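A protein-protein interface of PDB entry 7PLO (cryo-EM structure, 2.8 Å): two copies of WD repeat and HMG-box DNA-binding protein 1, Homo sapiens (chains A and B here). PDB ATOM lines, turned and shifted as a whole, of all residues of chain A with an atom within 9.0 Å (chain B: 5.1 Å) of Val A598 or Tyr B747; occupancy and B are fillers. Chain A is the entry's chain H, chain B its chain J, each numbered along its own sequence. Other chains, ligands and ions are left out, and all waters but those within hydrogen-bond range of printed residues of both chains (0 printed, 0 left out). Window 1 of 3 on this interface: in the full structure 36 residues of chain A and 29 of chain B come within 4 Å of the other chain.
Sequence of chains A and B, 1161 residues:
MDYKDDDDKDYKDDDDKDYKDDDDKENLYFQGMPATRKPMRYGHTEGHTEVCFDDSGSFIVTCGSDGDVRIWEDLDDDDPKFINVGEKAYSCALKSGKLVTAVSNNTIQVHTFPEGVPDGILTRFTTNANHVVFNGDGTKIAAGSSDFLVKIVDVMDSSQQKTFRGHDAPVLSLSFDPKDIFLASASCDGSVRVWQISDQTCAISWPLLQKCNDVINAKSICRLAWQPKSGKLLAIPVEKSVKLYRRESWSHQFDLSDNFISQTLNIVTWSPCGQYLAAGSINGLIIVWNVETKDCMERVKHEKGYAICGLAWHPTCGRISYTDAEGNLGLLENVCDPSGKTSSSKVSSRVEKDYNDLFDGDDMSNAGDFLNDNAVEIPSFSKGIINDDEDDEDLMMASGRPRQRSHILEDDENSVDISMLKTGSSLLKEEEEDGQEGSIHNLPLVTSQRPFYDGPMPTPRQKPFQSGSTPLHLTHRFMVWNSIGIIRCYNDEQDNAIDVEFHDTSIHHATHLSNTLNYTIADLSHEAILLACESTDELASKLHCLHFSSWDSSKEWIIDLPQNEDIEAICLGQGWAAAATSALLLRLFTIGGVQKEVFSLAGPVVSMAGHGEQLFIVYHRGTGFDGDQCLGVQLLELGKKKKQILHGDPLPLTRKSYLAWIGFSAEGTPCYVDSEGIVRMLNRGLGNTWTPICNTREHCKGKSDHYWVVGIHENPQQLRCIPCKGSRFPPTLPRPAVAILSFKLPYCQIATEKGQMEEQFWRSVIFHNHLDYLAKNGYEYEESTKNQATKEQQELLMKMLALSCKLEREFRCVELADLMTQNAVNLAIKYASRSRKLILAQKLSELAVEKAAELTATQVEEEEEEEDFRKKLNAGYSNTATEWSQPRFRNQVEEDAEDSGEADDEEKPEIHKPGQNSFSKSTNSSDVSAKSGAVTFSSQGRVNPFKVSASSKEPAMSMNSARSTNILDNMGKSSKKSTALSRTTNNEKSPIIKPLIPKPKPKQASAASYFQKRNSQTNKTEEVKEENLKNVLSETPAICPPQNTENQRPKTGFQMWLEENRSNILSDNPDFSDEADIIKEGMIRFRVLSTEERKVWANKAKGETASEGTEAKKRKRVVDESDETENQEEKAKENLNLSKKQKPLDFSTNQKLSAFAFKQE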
ATOM      1  N   ILE A 559     -23.326 -17.680  -4.504  1.00  0.00           N
ATOM      2  CA  ILE A 559     -23.510 -19.114  -4.301  1.00  0.00           C
ATOM      3  C   ILE A 559     -22.500 -19.582  -3.261  1.00  0.00           C
ATOM      4  O   ILE A 559     -21.420 -19.005  -3.121  1.00  0.00           O
ATOM      5  CB  ILE A 559     -23.378 -19.905  -5.629  1.00  0.00           C
ATOM      6  CG1 ILE A 559     -23.746 -21.378  -5.425  1.00  0.00           C
ATOM      7  CG2 ILE A 559     -21.965 -19.784  -6.225  1.00  0.00           C
ATOM      8  CD1 ILE A 559     -24.235 -22.065  -6.681  1.00  0.00           C
ATOM      9  N   ASP A 560     -22.867 -20.631  -2.520  1.00  0.00           N
ATOM     10  CA  ASP A 560     -22.035 -21.222  -1.476  1.00  0.00           C
ATOM     11  C   ASP A 560     -21.716 -22.668  -1.832  1.00  0.00           C
ATOM     12  O   ASP A 560     -22.585 -23.401  -2.314  1.00  0.00           O
ATOM     13  CB  ASP A 560     -22.739 -21.164  -0.115  1.00  0.00           C
ATOM     14  CG  ASP A 560     -24.089 -21.854  -0.125  1.00  0.00           C
ATOM     15  OD1 ASP A 560     -24.772 -21.809  -1.170  1.00  0.00           O
ATOM     16  OD2 ASP A 560     -24.467 -22.440   0.911  1.00  0.00           O
ATOM     17  N   LEU A 561     -20.452 -23.083  -1.582  1.00  0.00           N
ATOM     18  CA  LEU A 561     -19.956 -24.381  -2.017  1.00  0.00           C
ATOM     19  C   LEU A 561     -20.113 -25.422  -0.910  1.00  0.00           C
ATOM     20  O   LEU A 561     -20.329 -25.072   0.254  1.00  0.00           O
ATOM     21  CB  LEU A 561     -18.488 -24.259  -2.439  1.00  0.00           C
ATOM     22  CG  LEU A 561     -18.117 -23.471  -3.713  1.00  0.00           C
ATOM     23  CD1 LEU A 561     -18.941 -23.889  -4.936  1.00  0.00           C
ATOM     24  CD2 LEU A 561     -18.198 -21.956  -3.512  1.00  0.00           C
ATOM     25  N   PRO A 562     -20.015 -26.743  -1.239  1.00  0.00           N
ATOM     26  CA  PRO A 562     -20.294 -27.774  -0.222  1.00  0.00           C
ATOM     27  C   PRO A 562     -19.333 -27.787   0.959  1.00  0.00           C
ATOM     28  O   PRO A 562     -18.410 -26.970   1.042  1.00  0.00           O
ATOM     29  CB  PRO A 562     -20.192 -29.086  -1.015  1.00  0.00           C
ATOM     30  CG  PRO A 562     -20.395 -28.707  -2.423  1.00  0.00           C
ATOM     31  CD  PRO A 562     -19.778 -27.358  -2.560  1.00  0.00           C
ATOM     32  N   GLN A 563     -19.564 -28.724   1.881  1.00  0.00           N
ATOM     33  CA  GLN A 563     -18.829 -28.757   3.140  1.00  0.00           C
ATOM     34  C   GLN A 563     -17.344 -29.021   2.913  1.00  0.00           C
ATOM     35  O   GLN A 563     -16.960 -29.844   2.076  1.00  0.00           O
ATOM     36  CB  GLN A 563     -19.429 -29.820   4.082  1.00  0.00           C
ATOM     37  CG  GLN A 563     -19.131 -31.314   3.780  1.00  0.00           C
ATOM     38  CD  GLN A 563     -19.771 -31.819   2.500  1.00  0.00           C
ATOM     39  OE1 GLN A 563     -20.602 -31.139   1.897  1.00  0.00           O
ATOM     40  NE2 GLN A 563     -19.387 -33.020   2.081  1.00  0.00           N
ATOM     41  N   GLU A 565     -15.095 -27.475   1.432  1.00  0.00           N
ATOM     42  CA  GLU A 565     -14.521 -27.128   0.141  1.00  0.00           C
ATOM     43  C   GLU A 565     -13.912 -25.732   0.186  1.00  0.00           C
ATOM     44  O   GLU A 565     -14.362 -24.860   0.935  1.00  0.00           O
ATOM     45  CB  GLU A 565     -15.584 -27.206  -0.956  1.00  0.00           C
ATOM     46  CG  GLU A 565     -15.037 -27.026  -2.364  1.00  0.00           C
ATOM     47  CD  GLU A 565     -16.015 -27.461  -3.436  1.00  0.00           C
ATOM     48  OE1 GLU A 565     -16.579 -28.570  -3.318  1.00  0.00           O
ATOM     49  OE2 GLU A 565     -16.224 -26.694  -4.399  1.00  0.00           O
ATOM     50  N   ALA A 579     -13.988 -21.832 -11.621  1.00  0.00           N
ATOM     51  CA  ALA A 579     -13.272 -21.863 -10.353  1.00  0.00           C
ATOM     52  C   ALA A 579     -12.686 -23.253 -10.137  1.00  0.00           C
ATOM     53  O   ALA A 579     -13.384 -24.258 -10.308  1.00  0.00           O
ATOM     54  CB  ALA A 579     -14.201 -21.499  -9.189  1.00  0.00           C
ATOM     55  N   THR A 581     -11.173 -25.956  -7.400  1.00  0.00           N
ATOM     56  CA  THR A 581     -11.588 -26.248  -6.034  1.00  0.00           C
ATOM     57  C   THR A 581     -10.648 -27.265  -5.402  1.00  0.00           C
ATOM     58  O   THR A 581      -9.936 -28.002  -6.089  1.00  0.00           O
ATOM     59  CB  THR A 581     -13.029 -26.776  -5.997  1.00  0.00           C
ATOM     60  OG1 THR A 581     -13.077 -28.079  -6.589  1.00  0.00           O
ATOM     61  CG2 THR A 581     -13.967 -25.840  -6.760  1.00  0.00           C
ATOM     62  N   ALA A 583     -11.397 -29.958  -4.031  1.00  0.00           N
ATOM     63  CA  ALA A 583     -11.833 -31.325  -4.286  1.00  0.00           C
ATOM     64  C   ALA A 583     -11.213 -31.930  -5.546  1.00  0.00           C
ATOM     65  O   ALA A 583     -11.661 -32.999  -5.976  1.00  0.00           O
ATOM     66  CB  ALA A 583     -13.359 -31.371  -4.398  1.00  0.00           C
ATOM     67  N   LEU A 584     -10.193 -31.291  -6.131  1.00  0.00           N
ATOM     68  CA  LEU A 584      -9.638 -31.687  -7.427  1.00  0.00           C
ATOM     69  C   LEU A 584     -10.741 -31.725  -8.487  1.00  0.00           C
ATOM     70  O   LEU A 584     -10.796 -32.607  -9.350  1.00  0.00           O
ATOM     71  CB  LEU A 584      -8.874 -33.019  -7.321  1.00  0.00           C
ATOM     72  CG  LEU A 584      -7.414 -32.888  -6.856  1.00  0.00           C
ATOM     73  CD1 LEU A 584      -7.278 -32.214  -5.490  1.00  0.00           C
ATOM     74  CD2 LEU A 584      -6.740 -34.253  -6.835  1.00  0.00           C
ATOM     75  N   LEU A 585     -11.624 -30.726  -8.420  1.00  0.00           N
ATOM     76  CA  LEU A 585     -12.698 -30.517  -9.376  1.00  0.00           C
ATOM     77  C   LEU A 585     -12.644 -29.079  -9.876  1.00  0.00           C
ATOM     78  O   LEU A 585     -12.366 -28.148  -9.105  1.00  0.00           O
ATOM     79  CB  LEU A 585     -14.082 -30.789  -8.756  1.00  0.00           C
ATOM     80  CG  LEU A 585     -14.401 -32.176  -8.190  1.00  0.00           C
ATOM     81  CD1 LEU A 585     -15.750 -32.151  -7.488  1.00  0.00           C
ATOM     82  CD2 LEU A 585     -14.399 -33.233  -9.277  1.00  0.00           C
ATOM     83  N   LEU A 586     -12.906 -28.912 -11.171  1.00  0.00           N
ATOM     84  CA  LEU A 586     -13.175 -27.610 -11.760  1.00  0.00           C
ATOM     85  C   LEU A 586     -14.680 -27.448 -11.893  1.00  0.00           C
ATOM     86  O   LEU A 586     -15.370 -28.356 -12.393  1.00  0.00           O
ATOM     87  CB  LEU A 586     -12.514 -27.445 -13.129  1.00  0.00           C
ATOM     88  CG  LEU A 586     -12.397 -25.973 -13.553  1.00  0.00           C
ATOM     89  CD1 LEU A 586     -11.092 -25.378 -13.054  1.00  0.00           C
ATOM     90  CD2 LEU A 586     -12.527 -25.785 -15.054  1.00  0.00           C
ATOM     91  N   ARG A 587     -15.172 -26.297 -11.429  1.00  0.00           N
ATOM     92  CA  ARG A 587     -16.558 -25.881 -11.566  1.00  0.00           C
ATOM     93  C   ARG A 587     -16.620 -24.756 -12.586  1.00  0.00           C
ATOM     94  O   ARG A 587     -15.785 -23.850 -12.568  1.00  0.00           O
ATOM     95  CB  ARG A 587     -17.124 -25.404 -10.225  1.00  0.00           C
ATOM     96  CG  ARG A 587     -16.923 -26.388  -9.086  1.00  0.00           C
ATOM     97  CD  ARG A 587     -17.626 -25.939  -7.818  1.00  0.00           C
ATOM     98  NE  ARG A 587     -17.564 -26.970  -6.786  1.00  0.00           N
ATOM     99  CZ  ARG A 587     -18.299 -28.077  -6.768  1.00  0.00           C
ATOM    100  NH1 ARG A 587     -19.184 -28.345  -7.717  1.00  0.00           N
ATOM    101  NH2 ARG A 587     -18.137 -28.944  -5.773  1.00  0.00           N
ATOM    102  N   LEU A 588     -17.595 -24.833 -13.490  1.00  0.00           N
ATOM    103  CA  LEU A 588     -17.780 -23.855 -14.552  1.00  0.00           C
ATOM    104  C   LEU A 588     -19.225 -23.379 -14.528  1.00  0.00           C
ATOM    105  O   LEU A 588     -20.144 -24.176 -14.319  1.00  0.00           O
ATOM    106  CB  LEU A 588     -17.418 -24.459 -15.920  1.00  0.00           C
ATOM    107  CG  LEU A 588     -17.046 -23.488 -17.048  1.00  0.00           C
ATOM    108  CD1 LEU A 588     -15.948 -24.077 -17.923  1.00  0.00           C
ATOM    109  CD2 LEU A 588     -18.259 -23.130 -17.891  1.00  0.00           C
ATOM    110  N   PHE A 589     -19.413 -22.074 -14.727  1.00  0.00           N
ATOM    111  CA  PHE A 589     -20.700 -21.410 -14.590  1.00  0.00           C
ATOM    112  C   PHE A 589     -20.892 -20.441 -15.749  1.00  0.00           C
ATOM    113  O   PHE A 589     -20.010 -20.264 -16.592  1.00  0.00           O
ATOM    114  CB  PHE A 589     -20.805 -20.622 -13.276  1.00  0.00           C
ATOM    115  CG  PHE A 589     -20.254 -21.339 -12.078  1.00  0.00           C
ATOM    116  CD1 PHE A 589     -18.926 -21.188 -11.710  1.00  0.00           C
ATOM    117  CD2 PHE A 589     -21.071 -22.143 -11.305  1.00  0.00           C
ATOM    118  CE1 PHE A 589     -18.422 -21.841 -10.603  1.00  0.00           C
ATOM    119  CE2 PHE A 589     -20.573 -22.798 -10.196  1.00  0.00           C
ATOM    120  CZ  PHE A 589     -19.246 -22.645  -9.845  1.00  0.00           C
ATOM    121  N   GLY A 593     -25.276 -17.279 -13.491  1.00  0.00           N
ATOM    122  CA  GLY A 593     -25.409 -18.237 -12.412  1.00  0.00           C
ATOM    123  C   GLY A 593     -25.807 -19.647 -12.797  1.00  0.00           C
ATOM    124  O   GLY A 593     -26.063 -20.457 -11.900  1.00  0.00           O
ATOM    125  N   VAL A 594     -25.871 -19.970 -14.087  1.00  0.00           N
ATOM    126  CA  VAL A 594     -26.181 -21.333 -14.514  1.00  0.00           C
ATOM    127  C   VAL A 594     -24.940 -22.191 -14.327  1.00  0.00           C
ATOM    128  O   VAL A 594     -23.847 -21.820 -14.767  1.00  0.00           O
ATOM    129  CB  VAL A 594     -26.654 -21.365 -15.977  1.00  0.00           C
ATOM    130  CG1 VAL A 594     -26.861 -22.828 -16.440  1.00  0.00           C
ATOM    131  CG2 VAL A 594     -27.917 -20.506 -16.163  1.00  0.00           C
ATOM    132  N   GLN A 595     -25.104 -23.345 -13.684  1.00  0.00           N
ATOM    133  CA  GLN A 595     -23.988 -24.255 -13.460  1.00  0.00           C
ATOM    134  C   GLN A 595     -23.728 -25.065 -14.724  1.00  0.00           C
ATOM    135  O   GLN A 595     -24.611 -25.788 -15.197  1.00  0.00           O
ATOM    136  CB  GLN A 595     -24.275 -25.186 -12.286  1.00  0.00           C
ATOM    137  CG  GLN A 595     -24.594 -24.480 -10.976  1.00  0.00           C
ATOM    138  CD  GLN A 595     -24.514 -25.408  -9.777  1.00  0.00           C
ATOM    139  OE1 GLN A 595     -23.611 -26.239  -9.682  1.00  0.00           O
ATOM    140  NE2 GLN A 595     -25.461 -25.273  -8.857  1.00  0.00           N
ATOM    141  N   LYS A 596     -22.518 -24.942 -15.264  1.00  0.00           N
ATOM    142  CA  LYS A 596     -22.075 -25.731 -16.406  1.00  0.00           C
ATOM    143  C   LYS A 596     -21.397 -27.000 -15.882  1.00  0.00           C
ATOM    144  O   LYS A 596     -21.564 -27.363 -14.714  1.00  0.00           O
ATOM    145  CB  LYS A 596     -21.175 -24.879 -17.311  1.00  0.00           C
ATOM    146  CG  LYS A 596     -21.829 -23.606 -17.874  1.00  0.00           C
ATOM    147  CD  LYS A 596     -23.122 -23.855 -18.673  1.00  0.00           C
ATOM    148  CE  LYS A 596     -22.938 -24.803 -19.860  1.00  0.00           C
ATOM    149  NZ  LYS A 596     -21.909 -24.335 -20.828  1.00  0.00           N
ATOM    150  N   GLU A 597     -20.657 -27.702 -16.742  1.00  0.00           N
ATOM    151  CA  GLU A 597     -20.072 -28.988 -16.382  1.00  0.00           C
ATOM    152  C   GLU A 597     -19.097 -28.856 -15.218  1.00  0.00           C
ATOM    153  O   GLU A 597     -18.333 -27.891 -15.126  1.00  0.00           O
ATOM    154  CB  GLU A 597     -19.341 -29.596 -17.583  1.00  0.00           C
ATOM    155  CG  GLU A 597     -20.229 -29.964 -18.765  1.00  0.00           C
ATOM    156  CD  GLU A 597     -20.378 -28.836 -19.771  1.00  0.00           C
ATOM    157  OE1 GLU A 597     -20.277 -27.657 -19.368  1.00  0.00           O
ATOM    158  OE2 GLU A 597     -20.589 -29.129 -20.966  1.00  0.00           O
ATOM    159  N   VAL A 598     -19.142 -29.841 -14.322  1.00  0.00           N
ATOM    160  CA  VAL A 598     -18.156 -30.029 -13.263  1.00  0.00           C
ATOM    161  C   VAL A 598     -17.348 -31.260 -13.635  1.00  0.00           C
ATOM    162  O   VAL A 598     -17.927 -32.302 -13.969  1.00  0.00           O
ATOM    163  CB  VAL A 598     -18.827 -30.195 -11.886  1.00  0.00           C
ATOM    164  CG1 VAL A 598     -17.794 -30.518 -10.788  1.00  0.00           C
ATOM    165  CG2 VAL A 598     -19.629 -28.940 -11.526  1.00  0.00           C
ATOM    166  N   PHE A 599     -16.017 -31.145 -13.587  1.00  0.00           N
ATOM    167  CA  PHE A 599     -15.176 -32.259 -14.026  1.00  0.00           C
ATOM    168  C   PHE A 599     -13.901 -32.318 -13.197  1.00  0.00           C
ATOM    169  O   PHE A 599     -13.578 -31.401 -12.442  1.00  0.00           O
ATOM    170  CB  PHE A 599     -14.862 -32.175 -15.527  1.00  0.00           C
ATOM    171  CG  PHE A 599     -14.092 -30.952 -15.928  1.00  0.00           C
ATOM    172  CD1 PHE A 599     -14.743 -29.757 -16.177  1.00  0.00           C
ATOM    173  CD2 PHE A 599     -12.717 -31.005 -16.079  1.00  0.00           C
ATOM    174  CE1 PHE A 599     -14.038 -28.638 -16.558  1.00  0.00           C
ATOM    175  CE2 PHE A 599     -12.007 -29.887 -16.460  1.00  0.00           C
ATOM    176  CZ  PHE A 599     -12.668 -28.703 -16.701  1.00  0.00           C
ATOM    177  N   SER A 600     -13.188 -33.432 -13.342  1.00  0.00           N
ATOM    178  CA  SER A 600     -12.121 -33.828 -12.434  1.00  0.00           C
ATOM    179  C   SER A 600     -10.755 -33.382 -12.944  1.00  0.00           C
ATOM    180  O   SER A 600     -10.554 -33.150 -14.139  1.00  0.00           O
ATOM    181  CB  SER A 600     -12.127 -35.348 -12.240  1.00  0.00           C
ATOM    182  OG  SER A 600     -13.439 -35.828 -12.002  1.00  0.00           O
ATOM    183  N   LEU A 601      -9.810 -33.280 -12.005  1.00  0.00           N
ATOM    184  CA  LEU A 601      -8.446 -32.851 -12.285  1.00  0.00           C
ATOM    185  C   LEU A 601      -7.474 -33.772 -11.560  1.00  0.00           C
ATOM    186  O   LEU A 601      -7.819 -34.417 -10.568  1.00  0.00           O
ATOM    187  CB  LEU A 601      -8.218 -31.396 -11.852  1.00  0.00           C
ATOM    188  CG  LEU A 601      -9.181 -30.352 -12.425  1.00  0.00           C
ATOM    189  CD1 LEU A 601      -8.955 -29.020 -11.748  1.00  0.00           C
ATOM    190  CD2 LEU A 601      -9.014 -30.207 -13.931  1.00  0.00           C
ATOM    191  N   THR B 691     -15.804 -36.845 -15.750  1.00  0.00           N
ATOM    192  CA  THR B 691     -16.796 -36.184 -14.917  1.00  0.00           C
ATOM    193  C   THR B 691     -17.164 -37.076 -13.731  1.00  0.00           C
ATOM    194  O   THR B 691     -17.329 -38.289 -13.917  1.00  0.00           O
ATOM    195  CB  THR B 691     -18.070 -35.875 -15.715  1.00  0.00           C
ATOM    196  OG1 THR B 691     -18.525 -37.065 -16.372  1.00  0.00           O
ATOM    197  CG2 THR B 691     -17.813 -34.789 -16.747  1.00  0.00           C
ATOM    198  N   PRO B 692     -17.302 -36.544 -12.509  1.00  0.00           N
ATOM    199  CA  PRO B 692     -17.830 -37.378 -11.426  1.00  0.00           C
ATOM    200  C   PRO B 692     -19.309 -37.662 -11.629  1.00  0.00           C
ATOM    201  O   PRO B 692     -20.051 -36.840 -12.173  1.00  0.00           O
ATOM    202  CB  PRO B 692     -17.588 -36.534 -10.170  1.00  0.00           C
ATOM    203  CG  PRO B 692     -17.623 -35.148 -10.654  1.00  0.00           C
ATOM    204  CD  PRO B 692     -17.002 -35.182 -12.019  1.00  0.00           C
ATOM    205  N   LEU B 745     -24.378 -36.147  -8.288  1.00  0.00           N
ATOM    206  CA  LEU B 745     -23.259 -35.370  -8.815  1.00  0.00           C
ATOM    207  C   LEU B 745     -22.691 -34.439  -7.740  1.00  0.00           C
ATOM    208  O   LEU B 745     -23.455 -33.857  -6.965  1.00  0.00           O
ATOM    209  CB  LEU B 745     -23.705 -34.541 -10.015  1.00  0.00           C
ATOM    210  CG  LEU B 745     -24.605 -35.235 -11.047  1.00  0.00           C
ATOM    211  CD1 LEU B 745     -24.782 -34.340 -12.262  1.00  0.00           C
ATOM    212  CD2 LEU B 745     -24.068 -36.596 -11.472  1.00  0.00           C
ATOM    213  N   PRO B 746     -21.349 -34.245  -7.633  1.00  0.00           N
ATOM    214  CA  PRO B 746     -20.835 -33.201  -6.727  1.00  0.00           C
ATOM    215  C   PRO B 746     -21.029 -31.766  -7.218  1.00  0.00           C
ATOM    216  O   PRO B 746     -20.057 -31.019  -7.376  1.00  0.00           O
ATOM    217  CB  PRO B 746     -19.343 -33.557  -6.611  1.00  0.00           C
ATOM    218  CG  PRO B 746     -19.292 -35.002  -6.850  1.00  0.00           C
ATOM    219  CD  PRO B 746     -20.293 -35.230  -7.936  1.00  0.00           C
ATOM    220  N   TYR B 747     -22.276 -31.358  -7.435  1.00  0.00           N
ATOM    221  CA  TYR B 747     -22.605 -29.966  -7.702  1.00  0.00           C
ATOM    222  C   TYR B 747     -22.791 -29.228  -6.378  1.00  0.00           C
ATOM    223  O   TYR B 747     -22.805 -29.829  -5.302  1.00  0.00           O
ATOM    224  CB  TYR B 747     -23.860 -29.871  -8.575  1.00  0.00           C
ATOM    225  CG  TYR B 747     -23.582 -29.983 -10.062  1.00  0.00           C
ATOM    226  CD1 TYR B 747     -22.888 -31.067 -10.581  1.00  0.00           C
ATOM    227  CD2 TYR B 747     -24.022 -29.005 -10.944  1.00  0.00           C
ATOM    228  CE1 TYR B 747     -22.633 -31.171 -11.937  1.00  0.00           C
ATOM    229  CE2 TYR B 747     -23.773 -29.100 -12.301  1.00  0.00           C
ATOM    230  CZ  TYR B 747     -23.078 -30.185 -12.792  1.00  0.00           C
ATOM    231  OH  TYR B 747     -22.827 -30.286 -14.141  1.00  0.00           O
ATOM    232  N   CYS B 748     -22.917 -27.905  -6.462  1.00  0.00           N
ATOM    233  CA  CYS B 748     -23.113 -27.052  -5.300  1.00  0.00           C
ATOM    234  C   CYS B 748     -24.597 -26.760  -5.105  1.00  0.00           C
ATOM    235  O   CYS B 748     -25.382 -26.779  -6.056  1.00  0.00           O
ATOM    236  CB  CYS B 748     -22.334 -25.742  -5.443  1.00  0.00           C
ATOM    237  SG  CYS B 748     -22.423 -24.978  -7.078  1.00  0.00           S
ATOM    238  N   GLN B 749     -24.968 -26.487  -3.851  1.00  0.00           N
ATOM    239  CA  GLN B 749     -26.364 -26.281  -3.456  1.00  0.00           C
ATOM    240  C   GLN B 749     -27.218 -27.494  -3.824  1.00  0.00           C
ATOM    241  O   GLN B 749     -28.264 -27.381  -4.468  1.00  0.00           O
ATOM    242  CB  GLN B 749     -26.932 -24.998  -4.070  1.00  0.00           C
ATOM    243  CG  GLN B 749     -26.216 -23.734  -3.620  1.00  0.00           C
ATOM    244  CD  GLN B 749     -26.988 -22.473  -3.955  1.00  0.00           C
ATOM    245  OE1 GLN B 749     -27.843 -22.471  -4.842  1.00  0.00           O
ATOM    246  NE2 GLN B 749     -26.693 -21.391  -3.241  1.00  0.00           N
ATOM    247  N   ILE B 750     -26.754 -28.674  -3.404  1.00  0.00           N
ATOM    248  CA  ILE B 750     -27.466 -29.913  -3.710  1.00  0.00           C
ATOM    249  C   ILE B 750     -28.813 -29.960  -2.997  1.00  0.00           C
ATOM    250  O   ILE B 750     -29.772 -30.549  -3.510  1.00  0.00           O
ATOM    251  CB  ILE B 750     -26.590 -31.137  -3.363  1.00  0.00           C
ATOM    252  CG1 ILE B 750     -26.252 -31.202  -1.858  1.00  0.00           C
ATOM    253  CG2 ILE B 750     -25.317 -31.103  -4.197  1.00  0.00           C
ATOM    254  CD1 ILE B 750     -25.412 -32.409  -1.451  1.00  0.00           C
ATOM    255  N   GLU B 758     -30.804 -29.163 -11.893  1.00  0.00           N
ATOM    256  CA  GLU B 758     -29.541 -28.929 -12.592  1.00  0.00           C
ATOM    257  C   GLU B 758     -28.742 -30.225 -12.714  1.00  0.00           C
ATOM    258  O   GLU B 758     -28.226 -30.564 -13.794  1.00  0.00           O
ATOM    259  CB  GLU B 758     -28.742 -27.863 -11.839  1.00  0.00           C
ATOM    260  CG  GLU B 758     -27.489 -27.342 -12.534  1.00  0.00           C
ATOM    261  CD  GLU B 758     -27.794 -26.302 -13.593  1.00  0.00           C
ATOM    262  OE1 GLU B 758     -28.438 -26.649 -14.605  1.00  0.00           O
ATOM    263  OE2 GLU B 758     -27.394 -25.132 -13.409  1.00  0.00           O
ATOM    264  N   GLU B 759     -28.633 -30.963 -11.603  1.00  0.00           N
ATOM    265  CA  GLU B 759     -27.947 -32.250 -11.623  1.00  0.00           C
ATOM    266  C   GLU B 759     -28.633 -33.218 -12.576  1.00  0.00           C
ATOM    267  O   GLU B 759     -27.968 -33.979 -13.285  1.00  0.00           O
ATOM    268  CB  GLU B 759     -27.898 -32.848 -10.216  1.00  0.00           C
ATOM    269  CG  GLU B 759     -26.917 -32.178  -9.270  1.00  0.00           C
ATOM    270  CD  GLU B 759     -26.790 -32.919  -7.951  1.00  0.00           C
ATOM    271  OE1 GLU B 759     -26.680 -34.163  -7.972  1.00  0.00           O
ATOM    272  OE2 GLU B 759     -26.810 -32.258  -6.893  1.00  0.00           O
ATOM    273  N   TRP B 762     -27.702 -32.298 -16.234  1.00  0.00           N
ATOM    274  CA  TRP B 762     -26.356 -32.722 -16.599  1.00  0.00           C
ATOM    275  C   TRP B 762     -26.168 -34.232 -16.500  1.00  0.00           C
ATOM    276  O   TRP B 762     -25.183 -34.753 -17.034  1.00  0.00           O
ATOM    277  CB  TRP B 762     -25.329 -31.974 -15.745  1.00  0.00           C
ATOM    278  CG  TRP B 762     -25.246 -30.529 -16.144  1.00  0.00           C
ATOM    279  CD1 TRP B 762     -25.661 -29.449 -15.422  1.00  0.00           C
ATOM    280  CD2 TRP B 762     -24.747 -30.013 -17.385  1.00  0.00           C
ATOM    281  NE1 TRP B 762     -25.437 -28.291 -16.130  1.00  0.00           N
ATOM    282  CE2 TRP B 762     -24.878 -28.613 -17.340  1.00  0.00           C
ATOM    283  CE3 TRP B 762     -24.197 -30.602 -18.528  1.00  0.00           C
ATOM    284  CZ2 TRP B 762     -24.480 -27.792 -18.393  1.00  0.00           C
ATOM    285  CZ3 TRP B 762     -23.801 -29.785 -19.571  1.00  0.00           C
ATOM    286  CH2 TRP B 762     -23.943 -28.396 -19.496  1.00  0.00           C
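The side-chain amide nitrogen of Gln B749 is in hydrogen-bond range of the side-chain carboxylate of Asp A560 (2.9 Å). The guanidinium group (NH1) of Arg A587 sits at hydrogen-bond distance from the backbone carbonyl oxygen (O) of Pro B746, at 2.8 Å. The side-chain sulfur (SG) of Cys B748 sits at hydrogen-bond distance from the side-chain amide oxygen (OE1) of Gln A595, at 3.1 Å. The backbone NH of Gln A595 is in hydrogen-bond range of the side-chain carboxylate of Glu B758. O of Gln A595 is in hydrogen-bond range of NE1 of Trp B762, at 2.8 Å. The backbone carbonyl oxygen (O) of Lys A596 is in hydrogen-bond range of the side-chain hydroxyl (OH) of Tyr B747 (3.2 Å).
OE2 of Glu A565 lies within salt-bridge range of NE of Arg A587 (2.8 Å). The side-chain hydroxyl (OG1) of Thr A581 is in hydrogen-bond range of the backbone carbonyl oxygen (O) of Leu A585 (2.6 Å). N of Lys A596 lies within hydrogen-bond range of O of Leu A588 (2.7 Å).
CG1 of Ile A559 touches NE2 of Gln B749, at 3.7 Å. Leu A585 touches Pro B692 (CD2 to CG, 3.99 Å). CB of Pro B746 touches CD1 of Leu A585, at 3.96 Å. Tyr B747 touches Arg A587 (CA to NH1, 3.8 Å). Val A594 touches Glu B758 (CG1 to OE2, 3.8 Å). Thr B691 touches Val A598. Tyr B747 touches Val A598 (OH to N, 3.7 Å).
Of the printed residues of chain B, Leu A561 touches Cys B748 (3.9 Å). Of the printed residues of chain B, Val A598 touches Thr B691, Pro B692 and Tyr B747. Of chain A, only Leu A585 and Arg A587 come within 4 Å of Pro B746. Of chain A, only Pro A562, Arg A587, Gln A595, Lys A596, Glu A597 and Val A598 come within 4 Å of Tyr B747. Of the printed residues of chain A, Gln B749 touches Ile A559 (3.7 Å) and Asp A560 (2.9 Å). The nearest residue of chain B that does not touch Val A598 is Pro B746 (4.1 Å). The nearest residue of chain A that does not touch Tyr B747 is Leu A588 (6.4 Å). The nearest printed residue of chain B that does not touch Pro A562 is Cys B748 (4.2 Å).
Of the 11 printed residues of chain B, 8 touch a printed residue of chain A. Hydrophobic or aromatic side chains of chain B that line the printed part of chain A: Pro B692, Pro B746, Tyr B747 and Trp B762. Printed residues of chain A that touch a printed residue of chain B: Ile A559, Asp A560, Leu A561, Pro A562, Leu A585, Arg A587, Val A594, Gln A595, Lys A596, Glu A597, Val A598, Phe A599 and Ser A600. Hydrophobic or aromatic side chains of chain A within 4 Å of the printed part of chain B: Ile A559, Leu A561, Pro A562, Leu A585, Val A594 and Val A598.
No position is printed for both chains.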
